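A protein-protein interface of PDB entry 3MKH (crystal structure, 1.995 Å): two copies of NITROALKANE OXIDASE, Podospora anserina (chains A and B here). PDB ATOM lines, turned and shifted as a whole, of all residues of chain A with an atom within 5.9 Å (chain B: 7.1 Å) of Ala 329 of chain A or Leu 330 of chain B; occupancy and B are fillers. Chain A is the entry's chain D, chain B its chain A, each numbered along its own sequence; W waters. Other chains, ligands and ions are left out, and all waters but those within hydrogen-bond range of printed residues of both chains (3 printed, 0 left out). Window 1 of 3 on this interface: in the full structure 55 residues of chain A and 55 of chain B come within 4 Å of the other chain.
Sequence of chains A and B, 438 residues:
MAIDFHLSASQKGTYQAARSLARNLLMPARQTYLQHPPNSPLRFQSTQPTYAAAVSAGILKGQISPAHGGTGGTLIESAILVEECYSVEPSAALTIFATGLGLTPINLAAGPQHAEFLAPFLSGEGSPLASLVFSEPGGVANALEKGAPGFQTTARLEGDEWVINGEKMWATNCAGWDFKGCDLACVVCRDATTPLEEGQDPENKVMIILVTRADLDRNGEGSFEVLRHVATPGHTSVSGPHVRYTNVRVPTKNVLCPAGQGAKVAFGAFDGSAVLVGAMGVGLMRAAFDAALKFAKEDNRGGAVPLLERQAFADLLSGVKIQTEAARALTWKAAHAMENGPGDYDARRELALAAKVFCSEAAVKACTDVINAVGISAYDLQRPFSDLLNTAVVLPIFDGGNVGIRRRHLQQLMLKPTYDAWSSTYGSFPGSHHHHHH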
ATOM      1  N   PHE A   5      12.459  19.592  18.844  1.00  0.00           N
ATOM      2  CA  PHE A   5      12.259  19.015  20.174  1.00  0.00           C
ATOM      3  C   PHE A   5      10.777  18.926  20.580  1.00  0.00           C
ATOM      4  O   PHE A   5      10.455  18.590  21.722  1.00  0.00           O
ATOM      5  CB  PHE A   5      13.035  19.813  21.222  1.00  0.00           C
ATOM      6  CG  PHE A   5      14.518  19.620  21.153  1.00  0.00           C
ATOM      7  CD1 PHE A   5      15.292  20.374  20.281  1.00  0.00           C
ATOM      8  CD2 PHE A   5      15.143  18.691  21.968  1.00  0.00           C
ATOM      9  CE1 PHE A   5      16.678  20.197  20.215  1.00  0.00           C
ATOM     10  CE2 PHE A   5      16.525  18.512  21.911  1.00  0.00           C
ATOM     11  CZ  PHE A   5      17.285  19.266  21.028  1.00  0.00           C
ATOM     12  N   ILE A 322      19.237  22.163  35.858  1.00  0.00           N
ATOM     13  CA  ILE A 322      20.148  22.243  34.719  1.00  0.00           C
ATOM     14  C   ILE A 322      20.618  20.845  34.313  1.00  0.00           C
ATOM     15  O   ILE A 322      20.559  20.467  33.136  1.00  0.00           O
ATOM     16  CB  ILE A 322      21.392  23.122  35.045  1.00  0.00           C
ATOM     17  CG1 ILE A 322      20.982  24.583  35.286  1.00  0.00           C
ATOM     18  CG2 ILE A 322      22.420  23.049  33.921  1.00  0.00           C
ATOM     19  CD1 ILE A 322      22.105  25.445  35.861  1.00  0.00           C
ATOM     20  N   THR A 324      19.197  18.024  34.880  1.00  0.00           N
ATOM     21  CA  THR A 324      18.056  17.222  34.425  1.00  0.00           C
ATOM     22  C   THR A 324      17.738  17.515  32.966  1.00  0.00           C
ATOM     23  O   THR A 324      17.454  16.597  32.194  1.00  0.00           O
ATOM     24  CB  THR A 324      16.786  17.472  35.267  1.00  0.00           C
ATOM     25  OG1 THR A 324      17.075  17.217  36.643  1.00  0.00           O
ATOM     26  CG2 THR A 324      15.619  16.556  34.821  1.00  0.00           C
ATOM     27  N   GLU A 325      17.796  18.794  32.593  1.00  0.00           N
ATOM     28  CA  GLU A 325      17.547  19.186  31.212  1.00  0.00           C
ATOM     29  C   GLU A 325      18.632  18.665  30.280  1.00  0.00           C
ATOM     30  O   GLU A 325      18.341  18.188  29.188  1.00  0.00           O
ATOM     31  CB  GLU A 325      17.383  20.708  31.087  1.00  0.00           C
ATOM     32  CG  GLU A 325      16.251  21.271  31.928  1.00  0.00           C
ATOM     33  CD  GLU A 325      14.861  20.828  31.449  1.00  0.00           C
ATOM     34  OE1 GLU A 325      14.758  20.096  30.438  1.00  0.00           O
ATOM     35  OE2 GLU A 325      13.864  21.239  32.081  1.00  0.00           O
ATOM     36  N   ALA A 326      19.892  18.733  30.707  1.00  0.00           N
ATOM     37  CA  ALA A 326      20.959  18.145  29.910  1.00  0.00           C
ATOM     38  C   ALA A 326      20.757  16.632  29.764  1.00  0.00           C
ATOM     39  O   ALA A 326      20.930  16.066  28.675  1.00  0.00           O
ATOM     40  CB  ALA A 326      22.333  18.438  30.543  1.00  0.00           C
ATOM     41  N   ALA A 327      20.414  15.987  30.880  1.00  0.00           N
ATOM     42  CA  ALA A 327      20.217  14.538  30.921  1.00  0.00           C
ATOM     43  C   ALA A 327      19.134  14.092  29.932  1.00  0.00           C
ATOM     44  O   ALA A 327      19.345  13.152  29.164  1.00  0.00           O
ATOM     45  CB  ALA A 327      19.851  14.104  32.338  1.00  0.00           C
ATOM     46  N   ARG A 328      17.984  14.761  29.943  1.00  0.00           N
ATOM     47  CA  ARG A 328      16.918  14.409  28.999  1.00  0.00           C
ATOM     48  C   ARG A 328      17.290  14.703  27.546  1.00  0.00           C
ATOM     49  O   ARG A 328      17.002  13.900  26.646  1.00  0.00           O
ATOM     50  CB  ARG A 328      15.562  15.059  29.353  1.00  0.00           C
ATOM     51  CG  ARG A 328      14.362  14.436  28.572  1.00  0.00           C
ATOM     52  CD  ARG A 328      13.002  14.896  29.107  1.00  0.00           C
ATOM     53  NE  ARG A 328      13.153  16.273  29.484  1.00  0.00           N
ATOM     54  CZ  ARG A 328      12.954  16.765  30.689  1.00  0.00           C
ATOM     55  NH1 ARG A 328      12.496  16.013  31.682  1.00  0.00           N
ATOM     56  NH2 ARG A 328      13.199  18.047  30.873  1.00  0.00           N
ATOM     57  N   ALA A 329      17.914  15.851  27.303  1.00  0.00           N
ATOM     58  CA  ALA A 329      18.285  16.185  25.926  1.00  0.00           C
ATOM     59  C   ALA A 329      19.262  15.152  25.373  1.00  0.00           C
ATOM     60  O   ALA A 329      19.142  14.728  24.230  1.00  0.00           O
ATOM     61  CB  ALA A 329      18.858  17.616  25.828  1.00  0.00           C
ATOM     62  N   LEU A 330      20.212  14.726  26.198  1.00  0.00           N
ATOM     63  CA  LEU A 330      21.169  13.710  25.784  1.00  0.00           C
ATOM     64  C   LEU A 330      20.468  12.359  25.583  1.00  0.00           C
ATOM     65  O   LEU A 330      20.706  11.675  24.597  1.00  0.00           O
ATOM     66  CB  LEU A 330      22.302  13.563  26.808  1.00  0.00           C
ATOM     67  CG  LEU A 330      23.255  12.397  26.544  1.00  0.00           C
ATOM     68  CD1 LEU A 330      23.945  12.530  25.191  1.00  0.00           C
ATOM     69  CD2 LEU A 330      24.298  12.260  27.656  1.00  0.00           C
ATOM     70  N   THR A 331      19.615  11.983  26.528  1.00  0.00           N
ATOM     71  CA  THR A 331      18.847  10.737  26.411  1.00  0.00           C
ATOM     72  C   THR A 331      18.042  10.674  25.102  1.00  0.00           C
ATOM     73  O   THR A 331      18.128   9.697  24.359  1.00  0.00           O
ATOM     74  CB  THR A 331      17.928  10.550  27.613  1.00  0.00           C
ATOM     75  OG1 THR A 331      18.727  10.324  28.782  1.00  0.00           O
ATOM     76  CG2 THR A 331      16.982   9.354  27.405  1.00  0.00           C
ATOM     77  N   TRP A 332      17.291  11.727  24.799  1.00  0.00           N
ATOM     78  CA  TRP A 332      16.544  11.768  23.538  1.00  0.00           C
ATOM     79  C   TRP A 332      17.456  11.724  22.302  1.00  0.00           C
ATOM     80  O   TRP A 332      17.166  11.034  21.320  1.00  0.00           O
ATOM     81  CB  TRP A 332      15.632  12.986  23.484  1.00  0.00           C
ATOM     82  CG  TRP A 332      14.475  12.923  24.444  1.00  0.00           C
ATOM     83  CD1 TRP A 332      14.300  12.039  25.471  1.00  0.00           C
ATOM     84  CD2 TRP A 332      13.341  13.789  24.463  1.00  0.00           C
ATOM     85  NE1 TRP A 332      13.117  12.305  26.130  1.00  0.00           N
ATOM     86  CE2 TRP A 332      12.514  13.378  25.532  1.00  0.00           C
ATOM     87  CE3 TRP A 332      12.944  14.883  23.685  1.00  0.00           C
ATOM     88  CZ2 TRP A 332      11.313  14.020  25.838  1.00  0.00           C
ATOM     89  CZ3 TRP A 332      11.746  15.512  23.989  1.00  0.00           C
ATOM     90  CH2 TRP A 332      10.948  15.077  25.051  1.00  0.00           C
ATOM     91  N   LYS A 333      18.560  12.467  22.331  1.00  0.00           N
ATOM     92  CA  LYS A 333      19.520  12.367  21.235  1.00  0.00           C
ATOM     93  C   LYS A 333      19.995  10.928  21.010  1.00  0.00           C
ATOM     94  O   LYS A 333      20.053  10.458  19.874  1.00  0.00           O
ATOM     95  CB  LYS A 333      20.739  13.271  21.474  1.00  0.00           C
ATOM     96  CG  LYS A 333      21.893  12.987  20.526  1.00  0.00           C
ATOM     97  CD  LYS A 333      21.530  13.333  19.082  1.00  0.00           C
ATOM     98  CE  LYS A 333      22.664  12.946  18.141  1.00  0.00           C
ATOM     99  NZ  LYS A 333      22.427  13.293  16.710  1.00  0.00           N
ATOM    100  N   ALA A 334      20.358  10.238  22.087  1.00  0.00           N
ATOM    101  CA  ALA A 334      20.823   8.853  21.964  1.00  0.00           C
ATOM    102  C   ALA A 334      19.692   7.942  21.460  1.00  0.00           C
ATOM    103  O   ALA A 334      19.916   7.040  20.644  1.00  0.00           O
ATOM    104  CB  ALA A 334      21.348   8.349  23.295  1.00  0.00           C
ATOM    105  N   PHE B   5      16.638  14.836  15.592  1.00  0.00           N
ATOM    106  CA  PHE B   5      17.980  15.415  15.736  1.00  0.00           C
ATOM    107  C   PHE B   5      18.772  15.483  14.416  1.00  0.00           C
ATOM    108  O   PHE B   5      19.960  15.826  14.403  1.00  0.00           O
ATOM    109  CB  PHE B   5      18.779  14.649  16.805  1.00  0.00           C
ATOM    110  CG  PHE B   5      18.281  14.877  18.215  1.00  0.00           C
ATOM    111  CD1 PHE B   5      17.159  14.213  18.689  1.00  0.00           C
ATOM    112  CD2 PHE B   5      18.932  15.764  19.056  1.00  0.00           C
ATOM    113  CE1 PHE B   5      16.690  14.429  19.976  1.00  0.00           C
ATOM    114  CE2 PHE B   5      18.475  15.983  20.349  1.00  0.00           C
ATOM    115  CZ  PHE B   5      17.351  15.312  20.806  1.00  0.00           C
ATOM    116  N   VAL B 275      22.376  31.216  24.911  1.00  0.00           N
ATOM    117  CA  VAL B 275      22.324  30.018  24.070  1.00  0.00           C
ATOM    118  C   VAL B 275      23.628  29.883  23.291  1.00  0.00           C
ATOM    119  O   VAL B 275      24.202  28.800  23.187  1.00  0.00           O
ATOM    120  CB  VAL B 275      21.120  30.061  23.082  1.00  0.00           C
ATOM    121  CG1 VAL B 275      21.138  28.857  22.122  1.00  0.00           C
ATOM    122  CG2 VAL B 275      19.787  30.121  23.846  1.00  0.00           C
ATOM    123  N   THR B 324      30.468  16.695  26.364  1.00  0.00           N
ATOM    124  CA  THR B 324      30.313  17.472  25.132  1.00  0.00           C
ATOM    125  C   THR B 324      28.984  17.140  24.443  1.00  0.00           C
ATOM    126  O   THR B 324      28.290  18.027  23.946  1.00  0.00           O
ATOM    127  CB  THR B 324      31.487  17.253  24.148  1.00  0.00           C
ATOM    128  OG1 THR B 324      32.720  17.503  24.820  1.00  0.00           O
ATOM    129  CG2 THR B 324      31.397  18.226  22.960  1.00  0.00           C
ATOM    130  N   GLU B 325      28.642  15.858  24.408  1.00  0.00           N
ATOM    131  CA  GLU B 325      27.374  15.448  23.798  1.00  0.00           C
ATOM    132  C   GLU B 325      26.187  15.993  24.596  1.00  0.00           C
ATOM    133  O   GLU B 325      25.239  16.515  24.020  1.00  0.00           O
ATOM    134  CB  GLU B 325      27.311  13.919  23.624  1.00  0.00           C
ATOM    135  CG  GLU B 325      28.413  13.359  22.695  1.00  0.00           C
ATOM    136  CD  GLU B 325      28.283  13.860  21.255  1.00  0.00           C
ATOM    137  OE1 GLU B 325      27.331  14.604  20.962  1.00  0.00           O
ATOM    138  OE2 GLU B 325      29.116  13.486  20.406  1.00  0.00           O
ATOM    139  N   ALA B 326      26.248  15.915  25.926  1.00  0.00           N
ATOM    140  CA  ALA B 326      25.210  16.545  26.753  1.00  0.00           C
ATOM    141  C   ALA B 326      25.112  18.047  26.512  1.00  0.00           C
ATOM    142  O   ALA B 326      24.014  18.601  26.414  1.00  0.00           O
ATOM    143  CB  ALA B 326      25.477  16.287  28.228  1.00  0.00           C
ATOM    144  N   ALA B 327      26.266  18.714  26.457  1.00  0.00           N
ATOM    145  CA  ALA B 327      26.318  20.163  26.235  1.00  0.00           C
ATOM    146  C   ALA B 327      25.645  20.585  24.920  1.00  0.00           C
ATOM    147  O   ALA B 327      24.853  21.541  24.897  1.00  0.00           O
ATOM    148  CB  ALA B 327      27.794  20.677  26.275  1.00  0.00           C
ATOM    149  N   ARG B 328      25.971  19.896  23.830  1.00  0.00           N
ATOM    150  CA  ARG B 328      25.379  20.241  22.527  1.00  0.00           C
ATOM    151  C   ARG B 328      23.872  19.983  22.524  1.00  0.00           C
ATOM    152  O   ARG B 328      23.102  20.801  22.043  1.00  0.00           O
ATOM    153  CB  ARG B 328      26.034  19.499  21.345  1.00  0.00           C
ATOM    154  CG  ARG B 328      25.578  20.068  20.001  1.00  0.00           C
ATOM    155  CD  ARG B 328      26.091  19.266  18.803  1.00  0.00           C
ATOM    156  NE  ARG B 328      27.541  19.330  18.692  1.00  0.00           N
ATOM    157  CZ  ARG B 328      28.358  18.321  18.976  1.00  0.00           C
ATOM    158  NH1 ARG B 328      27.867  17.154  19.402  1.00  0.00           N
ATOM    159  NH2 ARG B 328      29.671  18.481  18.840  1.00  0.00           N
ATOM    160  N   ALA B 329      23.470  18.836  23.065  1.00  0.00           N
ATOM    161  CA  ALA B 329      22.058  18.463  23.155  1.00  0.00           C
ATOM    162  C   ALA B 329      21.265  19.529  23.909  1.00  0.00           C
ATOM    163  O   ALA B 329      20.199  19.964  23.453  1.00  0.00           O
ATOM    164  CB  ALA B 329      21.924  17.092  23.839  1.00  0.00           C
ATOM    165  N   LEU B 330      21.798  19.953  25.060  1.00  0.00           N
ATOM    166  CA  LEU B 330      21.177  20.995  25.869  1.00  0.00           C
ATOM    167  C   LEU B 330      21.147  22.333  25.127  1.00  0.00           C
ATOM    168  O   LEU B 330      20.124  23.021  25.115  1.00  0.00           O
ATOM    169  CB  LEU B 330      21.896  21.154  27.226  1.00  0.00           C
ATOM    170  CG  LEU B 330      21.315  22.288  28.087  1.00  0.00           C
ATOM    171  CD1 LEU B 330      19.837  22.071  28.309  1.00  0.00           C
ATOM    172  CD2 LEU B 330      22.030  22.414  29.429  1.00  0.00           C
ATOM    173  N   THR B 331      22.271  22.704  24.510  1.00  0.00           N
ATOM    174  CA  THR B 331      22.319  23.955  23.759  1.00  0.00           C
ATOM    175  C   THR B 331      21.258  23.972  22.643  1.00  0.00           C
ATOM    176  O   THR B 331      20.580  24.977  22.438  1.00  0.00           O
ATOM    177  CB  THR B 331      23.719  24.220  23.164  1.00  0.00           C
ATOM    178  OG1 THR B 331      24.643  24.462  24.229  1.00  0.00           O
ATOM    179  CG2 THR B 331      23.693  25.440  22.258  1.00  0.00           C
ATOM    180  N   TRP B 332      21.133  22.870  21.908  1.00  0.00           N
ATOM    181  CA  TRP B 332      20.159  22.824  20.802  1.00  0.00           C
ATOM    182  C   TRP B 332      18.710  22.840  21.309  1.00  0.00           C
ATOM    183  O   TRP B 332      17.828  23.455  20.701  1.00  0.00           O
ATOM    184  CB  TRP B 332      20.414  21.612  19.908  1.00  0.00           C
ATOM    185  CG  TRP B 332      21.642  21.770  19.033  1.00  0.00           C
ATOM    186  CD1 TRP B 332      22.608  22.738  19.131  1.00  0.00           C
ATOM    187  CD2 TRP B 332      22.018  20.946  17.924  1.00  0.00           C
ATOM    188  NE1 TRP B 332      23.565  22.560  18.152  1.00  0.00           N
ATOM    189  CE2 TRP B 332      23.225  21.469  17.399  1.00  0.00           C
ATOM    190  CE3 TRP B 332      21.450  19.818  17.319  1.00  0.00           C
ATOM    191  CZ2 TRP B 332      23.875  20.897  16.303  1.00  0.00           C
ATOM    192  CZ3 TRP B 332      22.101  19.247  16.233  1.00  0.00           C
ATOM    193  CH2 TRP B 332      23.298  19.793  15.735  1.00  0.00           C
ATOM    194  N   LYS B 333      18.459  22.162  22.423  1.00  0.00           N
ATOM    195  CA  LYS B 333      17.128  22.227  23.037  1.00  0.00           C
ATOM    196  C   LYS B 333      16.767  23.675  23.394  1.00  0.00           C
ATOM    197  O   LYS B 333      15.666  24.152  23.086  1.00  0.00           O
ATOM    198  CB  LYS B 333      17.040  21.303  24.266  1.00  0.00           C
ATOM    199  CG  LYS B 333      15.803  21.523  25.128  1.00  0.00           C
ATOM    200  CD  LYS B 333      14.507  21.214  24.383  1.00  0.00           C
ATOM    201  CE  LYS B 333      13.277  21.624  25.245  1.00  0.00           C
ATOM    202  NZ  LYS B 333      11.950  21.314  24.635  1.00  0.00           N
ATOM    203  N   ALA B 334      17.692  24.376  24.045  1.00  0.00           N
ATOM    204  CA  ALA B 334      17.474  25.770  24.410  1.00  0.00           C
ATOM    205  C   ALA B 334      17.294  26.634  23.165  1.00  0.00           C
ATOM    206  O   ALA B 334      16.449  27.523  23.144  1.00  0.00           O
ATOM    207  CB  ALA B 334      18.645  26.306  25.262  1.00  0.00           C
ATOM    208  N   ALA B 335      18.107  26.394  22.136  1.00  0.00           N
ATOM    209  CA  ALA B 335      17.969  27.146  20.890  1.00  0.00           C
ATOM    210  C   ALA B 335      16.554  26.957  20.320  1.00  0.00           C
ATOM    211  O   ALA B 335      15.891  27.911  19.896  1.00  0.00           O
ATOM    212  CB  ALA B 335      18.995  26.687  19.888  1.00  0.00           C
ATOM    213  N   HIS B 336      16.095  25.712  20.311  1.00  0.00           N
ATOM    214  CA  HIS B 336      14.795  25.404  19.721  1.00  0.00           C
ATOM    215  C   HIS B 336      13.658  25.988  20.565  1.00  0.00           C
ATOM    216  O   HIS B 336      12.736  26.620  20.035  1.00  0.00           O
ATOM    217  CB  HIS B 336      14.633  23.895  19.546  1.00  0.00           C
ATOM    218  CG  HIS B 336      13.372  23.509  18.843  1.00  0.00           C
ATOM    219  ND1 HIS B 336      12.244  23.082  19.512  1.00  0.00           N
ATOM    220  CD2 HIS B 336      13.046  23.527  17.525  1.00  0.00           C
ATOM    221  CE1 HIS B 336      11.285  22.828  18.634  1.00  0.00           C
ATOM    222  NE2 HIS B 336      11.748  23.088  17.421  1.00  0.00           N
ATOM    223  N   LEU B 351      15.802  27.626  29.992  1.00  0.00           N
ATOM    224  CA  LEU B 351      16.661  26.709  29.243  1.00  0.00           C
ATOM    225  C   LEU B 351      17.877  27.420  28.649  1.00  0.00           C
ATOM    226  O   LEU B 351      18.961  26.849  28.606  1.00  0.00           O
ATOM    227  CB  LEU B 351      15.878  25.998  28.137  1.00  0.00           C
ATOM    228  CG  LEU B 351      14.767  25.046  28.613  1.00  0.00           C
ATOM    229  CD1 LEU B 351      14.186  24.270  27.425  1.00  0.00           C
ATOM    230  CD2 LEU B 351      15.270  24.092  29.688  1.00  0.00           C
ATOM    231  N   ALA B 352      17.694  28.652  28.178  1.00  0.00           N
ATOM    232  CA  ALA B 352      18.825  29.427  27.669  1.00  0.00           C
ATOM    233  C   ALA B 352      19.859  29.619  28.776  1.00  0.00           C
ATOM    234  O   ALA B 352      21.027  29.348  28.575  1.00  0.00           O
ATOM    235  CB  ALA B 352      18.368  30.781  27.132  1.00  0.00           C
ATOM    236  N   LEU B 353      19.414  30.105  29.931  1.00  0.00           N
ATOM    237  CA  LEU B 353      20.274  30.232  31.110  1.00  0.00           C
ATOM    238  C   LEU B 353      20.963  28.916  31.477  1.00  0.00           C
ATOM    239  O   LEU B 353      22.167  28.889  31.792  1.00  0.00           O
ATOM    240  CB  LEU B 353      19.462  30.724  32.304  1.00  0.00           C
ATOM    241  CG  LEU B 353      18.815  32.099  32.129  1.00  0.00           C
ATOM    242  CD1 LEU B 353      17.692  32.307  33.153  1.00  0.00           C
ATOM    243  CD2 LEU B 353      19.870  33.173  32.252  1.00  0.00           C
ATOM    244  N   ALA B 354      20.210  27.823  31.438  1.00  0.00           N
ATOM    245  CA  ALA B 354      20.785  26.506  31.737  1.00  0.00           C
ATOM    246  C   ALA B 354      21.920  26.130  30.784  1.00  0.00           C
ATOM    247  O   ALA B 354      22.973  25.621  31.221  1.00  0.00           O
ATOM    248  CB  ALA B 354      19.696  25.423  31.720  1.00  0.00           C
ATOM    249  N   ALA B 355      21.717  26.359  29.485  1.00  0.00           N
ATOM    250  CA  ALA B 355      22.741  25.993  28.510  1.00  0.00           C
ATOM    251  C   ALA B 355      23.997  26.802  28.799  1.00  0.00           C
ATOM    252  O   ALA B 355      25.098  26.263  28.800  1.00  0.00           O
ATOM    253  CB  ALA B 355      22.274  26.241  27.059  1.00  0.00           C
ATOM    254  N   LYS B 356      23.820  28.097  29.045  1.00  0.00           N
ATOM    255  CA  LYS B 356      24.955  28.977  29.339  1.00  0.00           C
ATOM    256  C   LYS B 356      25.726  28.451  30.553  1.00  0.00           C
ATOM    257  O   LYS B 356      26.937  28.274  30.502  1.00  0.00           O
ATOM    258  CB  LYS B 356      24.480  30.414  29.585  1.00  0.00           C
ATOM    259  CG  LYS B 356      25.552  31.500  29.425  1.00  0.00           C
ATOM    260  CD  LYS B 356      26.518  31.590  30.617  1.00  0.00           C
ATOM    261  CE  LYS B 356      27.232  32.965  30.639  1.00  0.00           C
ATOM    262  NZ  LYS B 356      28.230  33.085  31.771  1.00  0.00           N
ATOM    263  N   VAL B 357      25.020  28.195  31.647  1.00  0.00           N
ATOM    264  CA  VAL B 357      25.688  27.756  32.862  1.00  0.00           C
ATOM    265  C   VAL B 357      26.316  26.371  32.707  1.00  0.00           C
ATOM    266  O   VAL B 357      27.455  26.154  33.104  1.00  0.00           O
ATOM    267  CB  VAL B 357      24.733  27.768  34.074  1.00  0.00           C
ATOM    268  CG1 VAL B 357      25.420  27.162  35.302  1.00  0.00           C
ATOM    269  CG2 VAL B 357      24.265  29.192  34.347  1.00  0.00           C
ATOM    270  N   PHE B 358      25.585  25.428  32.126  1.00  0.00           N
ATOM    271  CA  PHE B 358      26.097  24.058  32.019  1.00  0.00           C
ATOM    272  C   PHE B 358      27.344  23.976  31.136  1.00  0.00           C
ATOM    273  O   PHE B 358      28.343  23.377  31.513  1.00  0.00           O
ATOM    274  CB  PHE B 358      25.022  23.108  31.457  1.00  0.00           C
ATOM    275  CG  PHE B 358      25.505  21.681  31.260  1.00  0.00           C
ATOM    276  CD1 PHE B 358      26.094  21.288  30.066  1.00  0.00           C
ATOM    277  CD2 PHE B 358      25.396  20.749  32.280  1.00  0.00           C
ATOM    278  CE1 PHE B 358      26.540  19.973  29.880  1.00  0.00           C
ATOM    279  CE2 PHE B 358      25.837  19.446  32.108  1.00  0.00           C
ATOM    280  CZ  PHE B 358      26.411  19.052  30.904  1.00  0.00           C
ATOM    281  N   CYS B 359      27.246  24.560  29.942  1.00  0.00           N
ATOM    282  CA  CYS B 359      28.262  24.417  28.917  1.00  0.00           C
ATOM    283  C   CYS B 359      29.514  25.232  29.245  1.00  0.00           C
ATOM    284  O   CYS B 359      30.626  24.785  28.971  1.00  0.00           O
ATOM    285  CB  CYS B 359      27.713  24.826  27.541  1.00  0.00           C
ATOM    286  SG  CYS B 359      26.316  23.786  26.946  1.00  0.00           S
HETATM  287  O   HOH W   1      22.167  15.939  16.429  1.00  0.00           O
HETATM  288  O   HOH W   2      12.385  18.644  24.575  1.00  0.00           O
HETATM  289  O   HOH W   3       8.991  19.801  23.714  1.00  0.00           O
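Phe 5 of chain A touches Ala 329 of chain B, and with the chains exchanged Ala 329 of chain A touches Phe 5 of chain B.
Phe 5 of chain A touches Lys 333 of chain B, and with the chains exchanged Lys 333 of chain A touches Phe 5 of chain B.
Ala 329 of chain A touches its own counterpart, Ala 329 of chain B.
Ala 329 of chain A touches Leu 330 of chain B, and with the chains exchanged Leu 330 of chain A touches Ala 329 of chain B.
Of the 18 pairs that touch across the chains among the printed residues, 12 have their exchanged pair printed and touching as well.
OE1 of Glu 325 of chain B lies within salt-bridge range of NH1 of Arg 328 of chain B (3.0 Å).
The side-chain carboxylate of Glu 325 of chain A lies within salt-bridge range of the guanidinium group of Arg 328 of chain A (2.6 Å).
Of the printed residues of chain B, Phe 5 of chain A touches Phe 5 (3.5 Å), Ala 329 (3.9 Å), Trp 332 (3.5 Å), Lys 333 (3.4 Å) and His 336 (3.4 Å).
Ala 329 of chain A touches three residues of chain B.
Of the printed residues of chain B, Leu 330 of chain A touches Glu 325 (3.96 Å) and Ala 329 (3.8 Å).
Of the printed residues of chain B, Trp 332 of chain A touches Phe 5 (3.6 Å).
Printed residues of chain B within 4 Å of Lys 333 of chain A: Phe 5.
Val 275 of chain B touches none of the printed residues of chain A.
Leu 330 of chain B touches just these residues of chain A: Glu 325 (3.9 Å) and Ala 329 (3.8 Å).
Ala 335 of chain B touches none of the printed residues of chain A.
The nearest residue of chain A that does not touch Leu 330 of chain B is Ala 326 of chain A (4.1 Å).
Among the printed residues, pairs that only touch across the chains: Phe 5 of chain A with Phe 5 of chain B, Phe 5 of chain A with Ala 329 of chain B, Phe 5 of chain A with Trp 332 of chain B, Phe 5 of chain A with Lys 333 of chain B, Phe 5 of chain A with His 336 of chain B, Ile 322 of chain A with Ala 354 of chain B, Ile 322 of chain A with Val 357 of chain B, Ile 322 of chain A with Phe 358 of chain B, Glu 325 of chain A with Leu 330 of chain B, Glu 325 of chain A with Leu 351 of chain B, Ala 326 of chain A with Phe 358 of chain B, Ala 329 of chain A with Phe 5 of chain B, Ala 329 of chain A with Ala 329 of chain B, Ala 329 of chain A with Leu 330 of chain B, Leu 330 of chain A with Glu 325 of chain B, Leu 330 of chain A with Ala 329 of chain B, Trp 332 of chain A with Phe 5 of chain B and Lys 333 of chain A with Phe 5 of chain B.
Hydrophobic or aromatic side chains of chain B within 4 Å of the printed part of chain A: Phe 5, Ala 329, Leu 330, His 336, Leu 351, Ala 354, Val 357 and Phe 358.
Printed residues of chain A that touch a printed residue of chain B: Phe 5, Ile 322, Glu 325, Ala 326, Ala 329, Leu 330, Trp 332 and Lys 333.
Water W1 bridges the side-chain amino group of Lys 333 of chain A and the backbone carbonyl oxygen of Phe 5 of chain B.
Water W2 lies within hydrogen-bond range of the side-chain amino group (NZ) of Lys 333 of chain B (2.7 Å) and the backbone carbonyl oxygen (O) of Phe 5 of chain A (3.4 Å).
Water W3 bridges O of Phe 5 of chain A (2.8 Å) and NZ of Lys 333 of chain B (3.4 Å).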
